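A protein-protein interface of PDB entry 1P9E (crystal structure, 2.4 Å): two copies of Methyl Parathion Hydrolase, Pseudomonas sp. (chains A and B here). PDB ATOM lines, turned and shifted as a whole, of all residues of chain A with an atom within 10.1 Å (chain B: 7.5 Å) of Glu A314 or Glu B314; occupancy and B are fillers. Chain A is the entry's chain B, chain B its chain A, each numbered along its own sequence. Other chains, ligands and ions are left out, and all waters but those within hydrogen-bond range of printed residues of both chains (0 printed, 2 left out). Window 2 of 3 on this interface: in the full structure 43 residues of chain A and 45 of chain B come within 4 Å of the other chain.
Phe A88 touches Ile B311 (CZ to O, 3.5 Å).
CB of Arg B312 touches CZ of Phe A88, at 3.8 Å.
OE1 of Glu A314 is in salt-bridge range of NH1 of Arg A319 (2.6 Å).
O of Arg B312 sits at hydrogen-bond distance from N of Arg B319 (2.7 Å).
OE2 of Glu B314 lies within salt-bridge range of NH1 of Arg B319.
The backbone NH of Arg A319 sits at hydrogen-bond distance from the backbone carbonyl oxygen of Arg A312, at 2.9 Å.
Of the 22 printed residues of chain A, 4 touch a printed residue of chain B.
Printed residues of chain A that touch a printed residue of chain B: Lys A86, Phe A88, Glu A314 and Arg A319.
Of the 12 printed residues of chain B, 4 touch a printed residue of chain A.
Printed residues of chain B that touch a printed residue of chain A: Ile B311, Arg B312, Glu B314 and Arg B319.
Among the printed residues, 6 pairs touch across the chains.
Among the printed residues, Asp or Glu carboxylates within 4 Å of a Lys or Arg side-chain nitrogen of the other chain: Arg A319 with Glu B314 (2.7 Å).
Glu A314 touches its own counterpart, Glu B314.
Arg A319 touches Glu B314, but with the chains exchanged Glu A314 does not touch Arg B319 (4.6 Å).
Arg B319 touches its own counterpart, Arg A319.
Of the 6 pairs that touch across the chains among the printed residues, 2 have their exchanged pair printed and touching as well.
NH2 of Arg A319 sits close to NE of Arg B319 (3.0 Å).
NH1 of Arg A319 is in salt-bridge range of OE2 of Glu B314, 2.7 Å away.
OE2 of Glu B314 sits close to OE1 of Glu A314 (3.5 Å).
The guanidinium group (NE) of Arg B312 sits at hydrogen-bond distance from the backbone carbonyl oxygen (O) of Lys A86 (2.7 Å).
Of chain B, only Glu B314 (3.5 Å) comes within 4 Å of Glu A314.
Of the printed residues of chain B, Arg A319 touches Glu B314 and Arg B319.
Of the printed residues of chain A, Arg B312 touches Lys A86 and Phe A88.
No residue of chain A comes within 4 Å of Ala B313.
Of chain A, only Glu A314 (3.5 Å) and Arg A319 (2.7 Å) come within 4 Å of Glu B314.
No residue of chain A comes within 4 Å of Gly B317.
The nearest residue of chain B that does not touch Glu A314 is Arg B319 (4.6 Å).
The nearest printed residue of chain A that does not touch Arg B319 is Phe A320 (4.5 Å).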
ATOM      1  N   LYS A  86       6.286  21.153  -6.021  1.00  0.00           N
ATOM      2  CA  LYS A  86       5.863  21.631  -7.332  1.00  0.00           C
ATOM      3  C   LYS A  86       5.300  23.038  -7.197  1.00  0.00           C
ATOM      4  O   LYS A  86       5.271  23.800  -8.170  1.00  0.00           O
ATOM      5  CB  LYS A  86       4.824  20.682  -7.943  1.00  0.00           C
ATOM      6  CG  LYS A  86       5.336  19.239  -8.065  1.00  0.00           C
ATOM      7  CD  LYS A  86       4.256  18.284  -8.573  1.00  0.00           C
ATOM      8  CE  LYS A  86       4.728  16.834  -8.527  1.00  0.00           C
ATOM      9  NZ  LYS A  86       3.774  15.925  -9.232  1.00  0.00           N
ATOM     10  N   PHE A  88       6.632  25.213  -5.032  1.00  0.00           N
ATOM     11  CA  PHE A  88       7.690  25.980  -4.380  1.00  0.00           C
ATOM     12  C   PHE A  88       7.481  26.149  -2.895  1.00  0.00           C
ATOM     13  O   PHE A  88       7.816  27.192  -2.340  1.00  0.00           O
ATOM     14  CB  PHE A  88       7.789  27.364  -5.014  1.00  0.00           C
ATOM     15  CG  PHE A  88       8.095  27.324  -6.472  1.00  0.00           C
ATOM     16  CD1 PHE A  88       9.397  27.115  -6.916  1.00  0.00           C
ATOM     17  CD2 PHE A  88       7.079  27.437  -7.407  1.00  0.00           C
ATOM     18  CE1 PHE A  88       9.685  27.014  -8.291  1.00  0.00           C
ATOM     19  CE2 PHE A  88       7.353  27.339  -8.784  1.00  0.00           C
ATOM     20  CZ  PHE A  88       8.661  27.125  -9.222  1.00  0.00           C
ATOM     21  N   ALA A 260      -3.823  23.846  -0.248  1.00  0.00           N
ATOM     22  CA  ALA A 260      -4.042  24.187  -1.641  1.00  0.00           C
ATOM     23  C   ALA A 260      -3.120  23.468  -2.625  1.00  0.00           C
ATOM     24  O   ALA A 260      -3.531  23.108  -3.738  1.00  0.00           O
ATOM     25  CB  ALA A 260      -3.891  25.715  -1.826  1.00  0.00           C
ATOM     26  N   GLN A 263      -4.780  19.513  -2.425  1.00  0.00           N
ATOM     27  CA  GLN A 263      -6.208  19.330  -2.608  1.00  0.00           C
ATOM     28  C   GLN A 263      -6.953  19.938  -3.793  1.00  0.00           C
ATOM     29  O   GLN A 263      -8.116  19.592  -4.028  1.00  0.00           O
ATOM     30  CB  GLN A 263      -6.897  19.695  -1.292  1.00  0.00           C
ATOM     31  CG  GLN A 263      -6.410  18.819  -0.127  1.00  0.00           C
ATOM     32  CD  GLN A 263      -6.981  19.253   1.208  1.00  0.00           C
ATOM     33  OE1 GLN A 263      -6.885  20.427   1.589  1.00  0.00           O
ATOM     34  NE2 GLN A 263      -7.566  18.307   1.936  1.00  0.00           N
ATOM     35  N   PHE A 264      -6.320  20.841  -4.533  1.00  0.00           N
ATOM     36  CA  PHE A 264      -6.971  21.396  -5.708  1.00  0.00           C
ATOM     37  C   PHE A 264      -6.682  20.410  -6.838  1.00  0.00           C
ATOM     38  O   PHE A 264      -7.573  20.065  -7.612  1.00  0.00           O
ATOM     39  CB  PHE A 264      -6.418  22.782  -6.054  1.00  0.00           C
ATOM     40  CG  PHE A 264      -7.119  23.914  -5.348  1.00  0.00           C
ATOM     41  CD1 PHE A 264      -6.423  24.746  -4.463  1.00  0.00           C
ATOM     42  CD2 PHE A 264      -8.461  24.168  -5.588  1.00  0.00           C
ATOM     43  CE1 PHE A 264      -7.054  25.809  -3.836  1.00  0.00           C
ATOM     44  CE2 PHE A 264      -9.110  25.227  -4.965  1.00  0.00           C
ATOM     45  CZ  PHE A 264      -8.410  26.052  -4.089  1.00  0.00           C
ATOM     46  N   ASP A 265      -5.437  19.948  -6.930  1.00  0.00           N
ATOM     47  CA  ASP A 265      -5.075  18.976  -7.967  1.00  0.00           C
ATOM     48  C   ASP A 265      -5.667  17.601  -7.596  1.00  0.00           C
ATOM     49  O   ASP A 265      -5.884  16.750  -8.464  1.00  0.00           O
ATOM     50  CB  ASP A 265      -3.538  18.858  -8.108  1.00  0.00           C
ATOM     51  CG  ASP A 265      -2.914  19.941  -9.032  1.00  0.00           C
ATOM     52  OD1 ASP A 265      -1.673  20.154  -8.951  1.00  0.00           O
ATOM     53  OD2 ASP A 265      -3.634  20.567  -9.857  1.00  0.00           O
ATOM     54  N   ASP A 266      -5.934  17.387  -6.308  1.00  0.00           N
ATOM     55  CA  ASP A 266      -6.478  16.112  -5.854  1.00  0.00           C
ATOM     56  C   ASP A 266      -7.499  16.294  -4.737  1.00  0.00           C
ATOM     57  O   ASP A 266      -7.181  16.142  -3.547  1.00  0.00           O
ATOM     58  CB  ASP A 266      -5.352  15.205  -5.361  1.00  0.00           C
ATOM     59  CG  ASP A 266      -5.750  13.737  -5.330  1.00  0.00           C
ATOM     60  OD1 ASP A 266      -6.946  13.428  -5.580  1.00  0.00           O
ATOM     61  OD2 ASP A 266      -4.862  12.891  -5.056  1.00  0.00           O
ATOM     62  N   PRO A 267      -8.751  16.615  -5.110  1.00  0.00           N
ATOM     63  CA  PRO A 267      -9.872  16.829  -4.176  1.00  0.00           C
ATOM     64  C   PRO A 267     -10.143  15.623  -3.261  1.00  0.00           C
ATOM     65  O   PRO A 267     -10.822  15.761  -2.243  1.00  0.00           O
ATOM     66  CB  PRO A 267     -11.053  17.101  -5.105  1.00  0.00           C
ATOM     67  CG  PRO A 267     -10.400  17.676  -6.349  1.00  0.00           C
ATOM     68  CD  PRO A 267      -9.168  16.832  -6.509  1.00  0.00           C
ATOM     69  N   PHE A 288     -16.183  22.594  -5.368  1.00  0.00           N
ATOM     70  CA  PHE A 288     -15.323  22.869  -6.522  1.00  0.00           C
ATOM     71  C   PHE A 288     -16.024  22.725  -7.880  1.00  0.00           C
ATOM     72  O   PHE A 288     -15.846  23.571  -8.769  1.00  0.00           O
ATOM     73  CB  PHE A 288     -14.096  21.949  -6.502  1.00  0.00           C
ATOM     74  CG  PHE A 288     -13.147  22.213  -5.357  1.00  0.00           C
ATOM     75  CD1 PHE A 288     -13.322  23.315  -4.521  1.00  0.00           C
ATOM     76  CD2 PHE A 288     -12.066  21.363  -5.128  1.00  0.00           C
ATOM     77  CE1 PHE A 288     -12.437  23.568  -3.469  1.00  0.00           C
ATOM     78  CE2 PHE A 288     -11.168  21.604  -4.077  1.00  0.00           C
ATOM     79  CZ  PHE A 288     -11.351  22.703  -3.247  1.00  0.00           C
ATOM     80  N   ALA A 289     -16.798  21.647  -8.048  1.00  0.00           N
ATOM     81  CA  ALA A 289     -17.523  21.414  -9.293  1.00  0.00           C
ATOM     82  C   ALA A 289     -18.533  22.534  -9.502  1.00  0.00           C
ATOM     83  O   ALA A 289     -18.750  22.998 -10.621  1.00  0.00           O
ATOM     84  CB  ALA A 289     -18.245  20.082  -9.236  1.00  0.00           C
ATOM     85  N   ALA A 292     -16.844  25.855 -10.346  1.00  0.00           N
ATOM     86  CA  ALA A 292     -16.277  25.728 -11.684  1.00  0.00           C
ATOM     87  C   ALA A 292     -17.377  25.963 -12.717  1.00  0.00           C
ATOM     88  O   ALA A 292     -17.174  26.681 -13.691  1.00  0.00           O
ATOM     89  CB  ALA A 292     -15.676  24.342 -11.880  1.00  0.00           C
ATOM     90  N   ILE A 311     -12.497  29.206  -9.523  1.00  0.00           N
ATOM     91  CA  ILE A 311     -11.968  27.872  -9.695  1.00  0.00           C
ATOM     92  C   ILE A 311     -12.364  27.358 -11.063  1.00  0.00           C
ATOM     93  O   ILE A 311     -13.454  27.650 -11.554  1.00  0.00           O
ATOM     94  CB  ILE A 311     -12.515  26.938  -8.582  1.00  0.00           C
ATOM     95  CG1 ILE A 311     -11.922  27.364  -7.233  1.00  0.00           C
ATOM     96  CG2 ILE A 311     -12.186  25.489  -8.879  1.00  0.00           C
ATOM     97  CD1 ILE A 311     -12.184  26.377  -6.082  1.00  0.00           C
ATOM     98  N   ARG A 312     -11.466  26.626 -11.699  1.00  0.00           N
ATOM     99  CA  ARG A 312     -11.770  26.053 -13.002  1.00  0.00           C
ATOM    100  C   ARG A 312     -11.212  24.640 -13.029  1.00  0.00           C
ATOM    101  O   ARG A 312     -10.247  24.331 -12.332  1.00  0.00           O
ATOM    102  CB  ARG A 312     -11.150  26.875 -14.143  1.00  0.00           C
ATOM    103  CG  ARG A 312      -9.653  26.696 -14.360  1.00  0.00           C
ATOM    104  CD  ARG A 312      -9.253  27.199 -15.759  1.00  0.00           C
ATOM    105  NE  ARG A 312      -7.873  26.834 -16.088  1.00  0.00           N
ATOM    106  CZ  ARG A 312      -6.827  27.654 -15.986  1.00  0.00           C
ATOM    107  NH1 ARG A 312      -7.001  28.910 -15.572  1.00  0.00           N
ATOM    108  NH2 ARG A 312      -5.599  27.209 -16.278  1.00  0.00           N
ATOM    109  N   ALA A 313     -11.830  23.777 -13.819  1.00  0.00           N
ATOM    110  CA  ALA A 313     -11.350  22.415 -13.919  1.00  0.00           C
ATOM    111  C   ALA A 313     -10.074  22.357 -14.772  1.00  0.00           C
ATOM    112  O   ALA A 313      -9.948  23.056 -15.775  1.00  0.00           O
ATOM    113  CB  ALA A 313     -12.429  21.553 -14.527  1.00  0.00           C
ATOM    114  N   GLU A 314      -9.110  21.554 -14.345  1.00  0.00           N
ATOM    115  CA  GLU A 314      -7.880  21.387 -15.110  1.00  0.00           C
ATOM    116  C   GLU A 314      -7.567  19.917 -15.014  1.00  0.00           C
ATOM    117  O   GLU A 314      -7.147  19.426 -13.967  1.00  0.00           O
ATOM    118  CB  GLU A 314      -6.698  22.195 -14.548  1.00  0.00           C
ATOM    119  CG  GLU A 314      -5.573  22.402 -15.587  1.00  0.00           C
ATOM    120  CD  GLU A 314      -4.242  22.867 -14.986  1.00  0.00           C
ATOM    121  OE1 GLU A 314      -3.270  23.117 -15.757  1.00  0.00           O
ATOM    122  OE2 GLU A 314      -4.160  22.973 -13.741  1.00  0.00           O
ATOM    123  N   GLY A 315      -7.823  19.224 -16.116  1.00  0.00           N
ATOM    124  CA  GLY A 315      -7.588  17.796 -16.211  1.00  0.00           C
ATOM    125  C   GLY A 315      -8.245  16.928 -15.154  1.00  0.00           C
ATOM    126  O   GLY A 315      -9.466  16.762 -15.111  1.00  0.00           O
ATOM    127  N   LYS A 316      -7.397  16.365 -14.303  1.00  0.00           N
ATOM    128  CA  LYS A 316      -7.798  15.476 -13.222  1.00  0.00           C
ATOM    129  C   LYS A 316      -8.642  16.152 -12.143  1.00  0.00           C
ATOM    130  O   LYS A 316      -9.550  15.532 -11.595  1.00  0.00           O
ATOM    131  CB  LYS A 316      -6.538  14.906 -12.579  1.00  0.00           C
ATOM    132  CG  LYS A 316      -5.574  16.007 -12.125  1.00  0.00           C
ATOM    133  CD  LYS A 316      -4.361  15.434 -11.418  1.00  0.00           C
ATOM    134  CE  LYS A 316      -3.485  16.517 -10.823  1.00  0.00           C
ATOM    135  NZ  LYS A 316      -2.394  15.877 -10.016  1.00  0.00           N
ATOM    136  N   GLY A 317      -8.328  17.411 -11.832  1.00  0.00           N
ATOM    137  CA  GLY A 317      -9.050  18.125 -10.786  1.00  0.00           C
ATOM    138  C   GLY A 317      -9.288  19.614 -10.991  1.00  0.00           C
ATOM    139  O   GLY A 317      -9.916  20.010 -11.974  1.00  0.00           O
ATOM    140  N   TYR A 318      -8.805  20.454 -10.075  1.00  0.00           N
ATOM    141  CA  TYR A 318      -9.035  21.895 -10.205  1.00  0.00           C
ATOM    142  C   TYR A 318      -7.824  22.816 -10.150  1.00  0.00           C
ATOM    143  O   TYR A 318      -6.719  22.405  -9.826  1.00  0.00           O
ATOM    144  CB  TYR A 318     -10.066  22.353  -9.164  1.00  0.00           C
ATOM    145  CG  TYR A 318     -11.387  21.623  -9.281  1.00  0.00           C
ATOM    146  CD1 TYR A 318     -11.572  20.376  -8.679  1.00  0.00           C
ATOM    147  CD2 TYR A 318     -12.414  22.129 -10.073  1.00  0.00           C
ATOM    148  CE1 TYR A 318     -12.733  19.643  -8.869  1.00  0.00           C
ATOM    149  CE2 TYR A 318     -13.593  21.405 -10.275  1.00  0.00           C
ATOM    150  CZ  TYR A 318     -13.738  20.161  -9.672  1.00  0.00           C
ATOM    151  OH  TYR A 318     -14.880  19.420  -9.902  1.00  0.00           O
ATOM    152  N   ARG A 319      -8.055  24.078 -10.481  1.00  0.00           N
ATOM    153  CA  ARG A 319      -7.014  25.107 -10.485  1.00  0.00           C
ATOM    154  C   ARG A 319      -7.620  26.350  -9.836  1.00  0.00           C
ATOM    155  O   ARG A 319      -8.665  26.845 -10.283  1.00  0.00           O
ATOM    156  CB  ARG A 319      -6.596  25.405 -11.932  1.00  0.00           C
ATOM    157  CG  ARG A 319      -5.474  26.421 -12.152  1.00  0.00           C
ATOM    158  CD  ARG A 319      -4.728  26.042 -13.448  1.00  0.00           C
ATOM    159  NE  ARG A 319      -3.770  27.041 -13.928  1.00  0.00           N
ATOM    160  CZ  ARG A 319      -2.777  26.786 -14.792  1.00  0.00           C
ATOM    161  NH1 ARG A 319      -2.591  25.556 -15.277  1.00  0.00           N
ATOM    162  NH2 ARG A 319      -1.971  27.770 -15.189  1.00  0.00           N
ATOM    163  N   PHE A 320      -6.987  26.844  -8.773  1.00  0.00           N
ATOM    164  CA  PHE A 320      -7.489  28.040  -8.088  1.00  0.00           C
ATOM    165  C   PHE A 320      -6.896  29.307  -8.698  1.00  0.00           C
ATOM    166  O   PHE A 320      -5.674  29.441  -8.792  1.00  0.00           O
ATOM    167  CB  PHE A 320      -7.128  27.978  -6.608  1.00  0.00           C
ATOM    168  CG  PHE A 320      -7.578  29.174  -5.813  1.00  0.00           C
ATOM    169  CD1 PHE A 320      -8.924  29.353  -5.488  1.00  0.00           C
ATOM    170  CD2 PHE A 320      -6.644  30.111  -5.358  1.00  0.00           C
ATOM    171  CE1 PHE A 320      -9.335  30.450  -4.720  1.00  0.00           C
ATOM    172  CE2 PHE A 320      -7.044  31.210  -4.587  1.00  0.00           C
ATOM    173  CZ  PHE A 320      -8.395  31.380  -4.269  1.00  0.00           C
ATOM    174  N   VAL A 321      -7.756  30.230  -9.123  1.00  0.00           N
ATOM    175  CA  VAL A 321      -7.305  31.503  -9.694  1.00  0.00           C
ATOM    176  C   VAL A 321      -7.676  32.592  -8.661  1.00  0.00           C
ATOM    177  O   VAL A 321      -8.846  32.965  -8.526  1.00  0.00           O
ATOM    178  CB  VAL A 321      -8.005  31.769 -11.070  1.00  0.00           C
ATOM    179  CG1 VAL A 321      -7.411  33.004 -11.762  1.00  0.00           C
ATOM    180  CG2 VAL A 321      -7.839  30.559 -11.976  1.00  0.00           C
ATOM    181  N   PHE B 264       2.346  34.148 -19.914  1.00  0.00           N
ATOM    182  CA  PHE B 264       3.045  33.105 -19.158  1.00  0.00           C
ATOM    183  C   PHE B 264       2.850  31.815 -19.961  1.00  0.00           C
ATOM    184  O   PHE B 264       3.792  31.042 -20.162  1.00  0.00           O
ATOM    185  CB  PHE B 264       2.474  32.922 -17.745  1.00  0.00           C
ATOM    186  CG  PHE B 264       3.022  33.899 -16.734  1.00  0.00           C
ATOM    187  CD1 PHE B 264       2.194  34.840 -16.130  1.00  0.00           C
ATOM    188  CD2 PHE B 264       4.368  33.867 -16.378  1.00  0.00           C
ATOM    189  CE1 PHE B 264       2.709  35.741 -15.178  1.00  0.00           C
ATOM    190  CE2 PHE B 264       4.889  34.757 -15.434  1.00  0.00           C
ATOM    191  CZ  PHE B 264       4.056  35.696 -14.835  1.00  0.00           C
ATOM    192  N   ASP B 265       1.622  31.596 -20.430  1.00  0.00           N
ATOM    193  CA  ASP B 265       1.317  30.410 -21.211  1.00  0.00           C
ATOM    194  C   ASP B 265       1.995  30.526 -22.569  1.00  0.00           C
ATOM    195  O   ASP B 265       2.576  29.547 -23.041  1.00  0.00           O
ATOM    196  CB  ASP B 265      -0.206  30.206 -21.325  1.00  0.00           C
ATOM    197  CG  ASP B 265      -0.836  29.717 -19.990  1.00  0.00           C
ATOM    198  OD1 ASP B 265      -0.526  28.580 -19.540  1.00  0.00           O
ATOM    199  OD2 ASP B 265      -1.630  30.468 -19.376  1.00  0.00           O
ATOM    200  N   ILE B 311       8.141  30.726 -10.715  1.00  0.00           N
ATOM    201  CA  ILE B 311       7.700  30.317 -12.028  1.00  0.00           C
ATOM    202  C   ILE B 311       8.215  28.930 -12.394  1.00  0.00           C
ATOM    203  O   ILE B 311       9.396  28.635 -12.260  1.00  0.00           O
ATOM    204  CB  ILE B 311       8.124  31.353 -13.096  1.00  0.00           C
ATOM    205  CG1 ILE B 311       7.665  30.894 -14.470  1.00  0.00           C
ATOM    206  CG2 ILE B 311       9.633  31.551 -13.084  1.00  0.00           C
ATOM    207  CD1 ILE B 311       7.679  32.005 -15.461  1.00  0.00           C
ATOM    208  N   ARG B 312       7.311  28.062 -12.830  1.00  0.00           N
ATOM    209  CA  ARG B 312       7.698  26.712 -13.226  1.00  0.00           C
ATOM    210  C   ARG B 312       7.260  26.460 -14.673  1.00  0.00           C
ATOM    211  O   ARG B 312       6.355  27.135 -15.194  1.00  0.00           O
ATOM    212  CB  ARG B 312       7.046  25.665 -12.306  1.00  0.00           C
ATOM    213  CG  ARG B 312       5.514  25.601 -12.417  1.00  0.00           C
ATOM    214  CD  ARG B 312       4.967  24.289 -11.856  1.00  0.00           C
ATOM    215  NE  ARG B 312       4.221  24.456 -10.612  1.00  0.00           N
ATOM    216  CZ  ARG B 312       2.921  24.722 -10.552  1.00  0.00           C
ATOM    217  NH1 ARG B 312       2.225  24.849 -11.682  1.00  0.00           N
ATOM    218  NH2 ARG B 312       2.316  24.860  -9.369  1.00  0.00           N
ATOM    219  N   ALA B 313       7.915  25.491 -15.308  1.00  0.00           N
ATOM    220  CA  ALA B 313       7.605  25.101 -16.679  1.00  0.00           C
ATOM    221  C   ALA B 313       6.231  24.420 -16.710  1.00  0.00           C
ATOM    222  O   ALA B 313       5.839  23.743 -15.761  1.00  0.00           O
ATOM    223  CB  ALA B 313       8.669  24.150 -17.186  1.00  0.00           C
ATOM    224  N   GLU B 314       5.485  24.618 -17.787  1.00  0.00           N
ATOM    225  CA  GLU B 314       4.164  24.009 -17.912  1.00  0.00           C
ATOM    226  C   GLU B 314       3.871  23.824 -19.387  1.00  0.00           C
ATOM    227  O   GLU B 314       3.502  24.779 -20.076  1.00  0.00           O
ATOM    228  CB  GLU B 314       3.083  24.897 -17.278  1.00  0.00           C
ATOM    229  CG  GLU B 314       1.652  24.369 -17.479  1.00  0.00           C
ATOM    230  CD  GLU B 314       0.578  25.173 -16.717  1.00  0.00           C
ATOM    231  OE1 GLU B 314       0.432  26.400 -16.968  1.00  0.00           O
ATOM    232  OE2 GLU B 314      -0.132  24.568 -15.874  1.00  0.00           O
ATOM    233  N   GLY B 315       4.054  22.595 -19.870  1.00  0.00           N
ATOM    234  CA  GLY B 315       3.814  22.288 -21.271  1.00  0.00           C
ATOM    235  C   GLY B 315       4.351  23.311 -22.260  1.00  0.00           C
ATOM    236  O   GLY B 315       5.561  23.433 -22.467  1.00  0.00           O
ATOM    237  N   LYS B 316       3.442  24.051 -22.878  1.00  0.00           N
ATOM    238  CA  LYS B 316       3.819  25.060 -23.857  1.00  0.00           C
ATOM    239  C   LYS B 316       4.735  26.136 -23.272  1.00  0.00           C
ATOM    240  O   LYS B 316       5.772  26.471 -23.852  1.00  0.00           O
ATOM    241  CB  LYS B 316       2.553  25.721 -24.440  1.00  0.00           C
ATOM    242  CG  LYS B 316       1.654  26.454 -23.403  1.00  0.00           C
ATOM    243  CD  LYS B 316       0.280  26.848 -24.000  1.00  0.00           C
ATOM    244  CE  LYS B 316       0.394  27.604 -25.347  1.00  0.00           C
ATOM    245  NZ  LYS B 316      -0.942  28.059 -25.866  1.00  0.00           N
ATOM    246  N   GLY B 317       4.357  26.672 -22.113  1.00  0.00           N
ATOM    247  CA  GLY B 317       5.155  27.734 -21.528  1.00  0.00           C
ATOM    248  C   GLY B 317       5.456  27.662 -20.051  1.00  0.00           C
ATOM    249  O   GLY B 317       6.205  26.787 -19.607  1.00  0.00           O
ATOM    250  N   TYR B 318       4.882  28.587 -19.284  1.00  0.00           N
ATOM    251  CA  TYR B 318       5.143  28.636 -17.852  1.00  0.00           C
ATOM    252  C   TYR B 318       3.929  28.862 -16.980  1.00  0.00           C
ATOM    253  O   TYR B 318       2.891  29.332 -17.434  1.00  0.00           O
ATOM    254  CB  TYR B 318       6.164  29.732 -17.541  1.00  0.00           C
ATOM    255  CG  TYR B 318       7.487  29.548 -18.237  1.00  0.00           C
ATOM    256  CD1 TYR B 318       7.657  29.936 -19.571  1.00  0.00           C
ATOM    257  CD2 TYR B 318       8.563  28.938 -17.583  1.00  0.00           C
ATOM    258  CE1 TYR B 318       8.868  29.711 -20.240  1.00  0.00           C
ATOM    259  CE2 TYR B 318       9.778  28.710 -18.247  1.00  0.00           C
ATOM    260  CZ  TYR B 318       9.917  29.093 -19.573  1.00  0.00           C
ATOM    261  OH  TYR B 318      11.087  28.814 -20.249  1.00  0.00           O
ATOM    262  N   ARG B 319       4.069  28.508 -15.712  1.00  0.00           N
ATOM    263  CA  ARG B 319       2.997  28.717 -14.759  1.00  0.00           C
ATOM    264  C   ARG B 319       3.555  29.658 -13.708  1.00  0.00           C
ATOM    265  O   ARG B 319       4.576  29.360 -13.096  1.00  0.00           O
ATOM    266  CB  ARG B 319       2.579  27.400 -14.101  1.00  0.00           C
ATOM    267  CG  ARG B 319       1.537  27.554 -13.000  1.00  0.00           C
ATOM    268  CD  ARG B 319       0.356  28.396 -13.479  1.00  0.00           C
ATOM    269  NE  ARG B 319      -0.747  28.424 -12.519  1.00  0.00           N
ATOM    270  CZ  ARG B 319      -1.397  27.339 -12.104  1.00  0.00           C
ATOM    271  NH1 ARG B 319      -1.052  26.133 -12.566  1.00  0.00           N
ATOM    272  NH2 ARG B 319      -2.396  27.453 -11.232  1.00  0.00           N
ATOM    273  N   PHE B 320       2.902  30.798 -13.510  1.00  0.00           N
ATOM    274  CA  PHE B 320       3.342  31.769 -12.507  1.00  0.00           C
ATOM    275  C   PHE B 320       2.742  31.382 -11.162  1.00  0.00           C
ATOM    276  O   PHE B 320       1.546  31.125 -11.068  1.00  0.00           O
ATOM    277  CB  PHE B 320       2.871  33.166 -12.894  1.00  0.00           C
ATOM    278  CG  PHE B 320       3.192  34.217 -11.880  1.00  0.00           C
ATOM    279  CD1 PHE B 320       4.518  34.498 -11.538  1.00  0.00           C
ATOM    280  CD2 PHE B 320       2.172  34.949 -11.274  1.00  0.00           C
ATOM    281  CE1 PHE B 320       4.813  35.499 -10.605  1.00  0.00           C
ATOM    282  CE2 PHE B 320       2.455  35.952 -10.340  1.00  0.00           C
ATOM    283  CZ  PHE B 320       3.770  36.229 -10.005  1.00  0.00           C
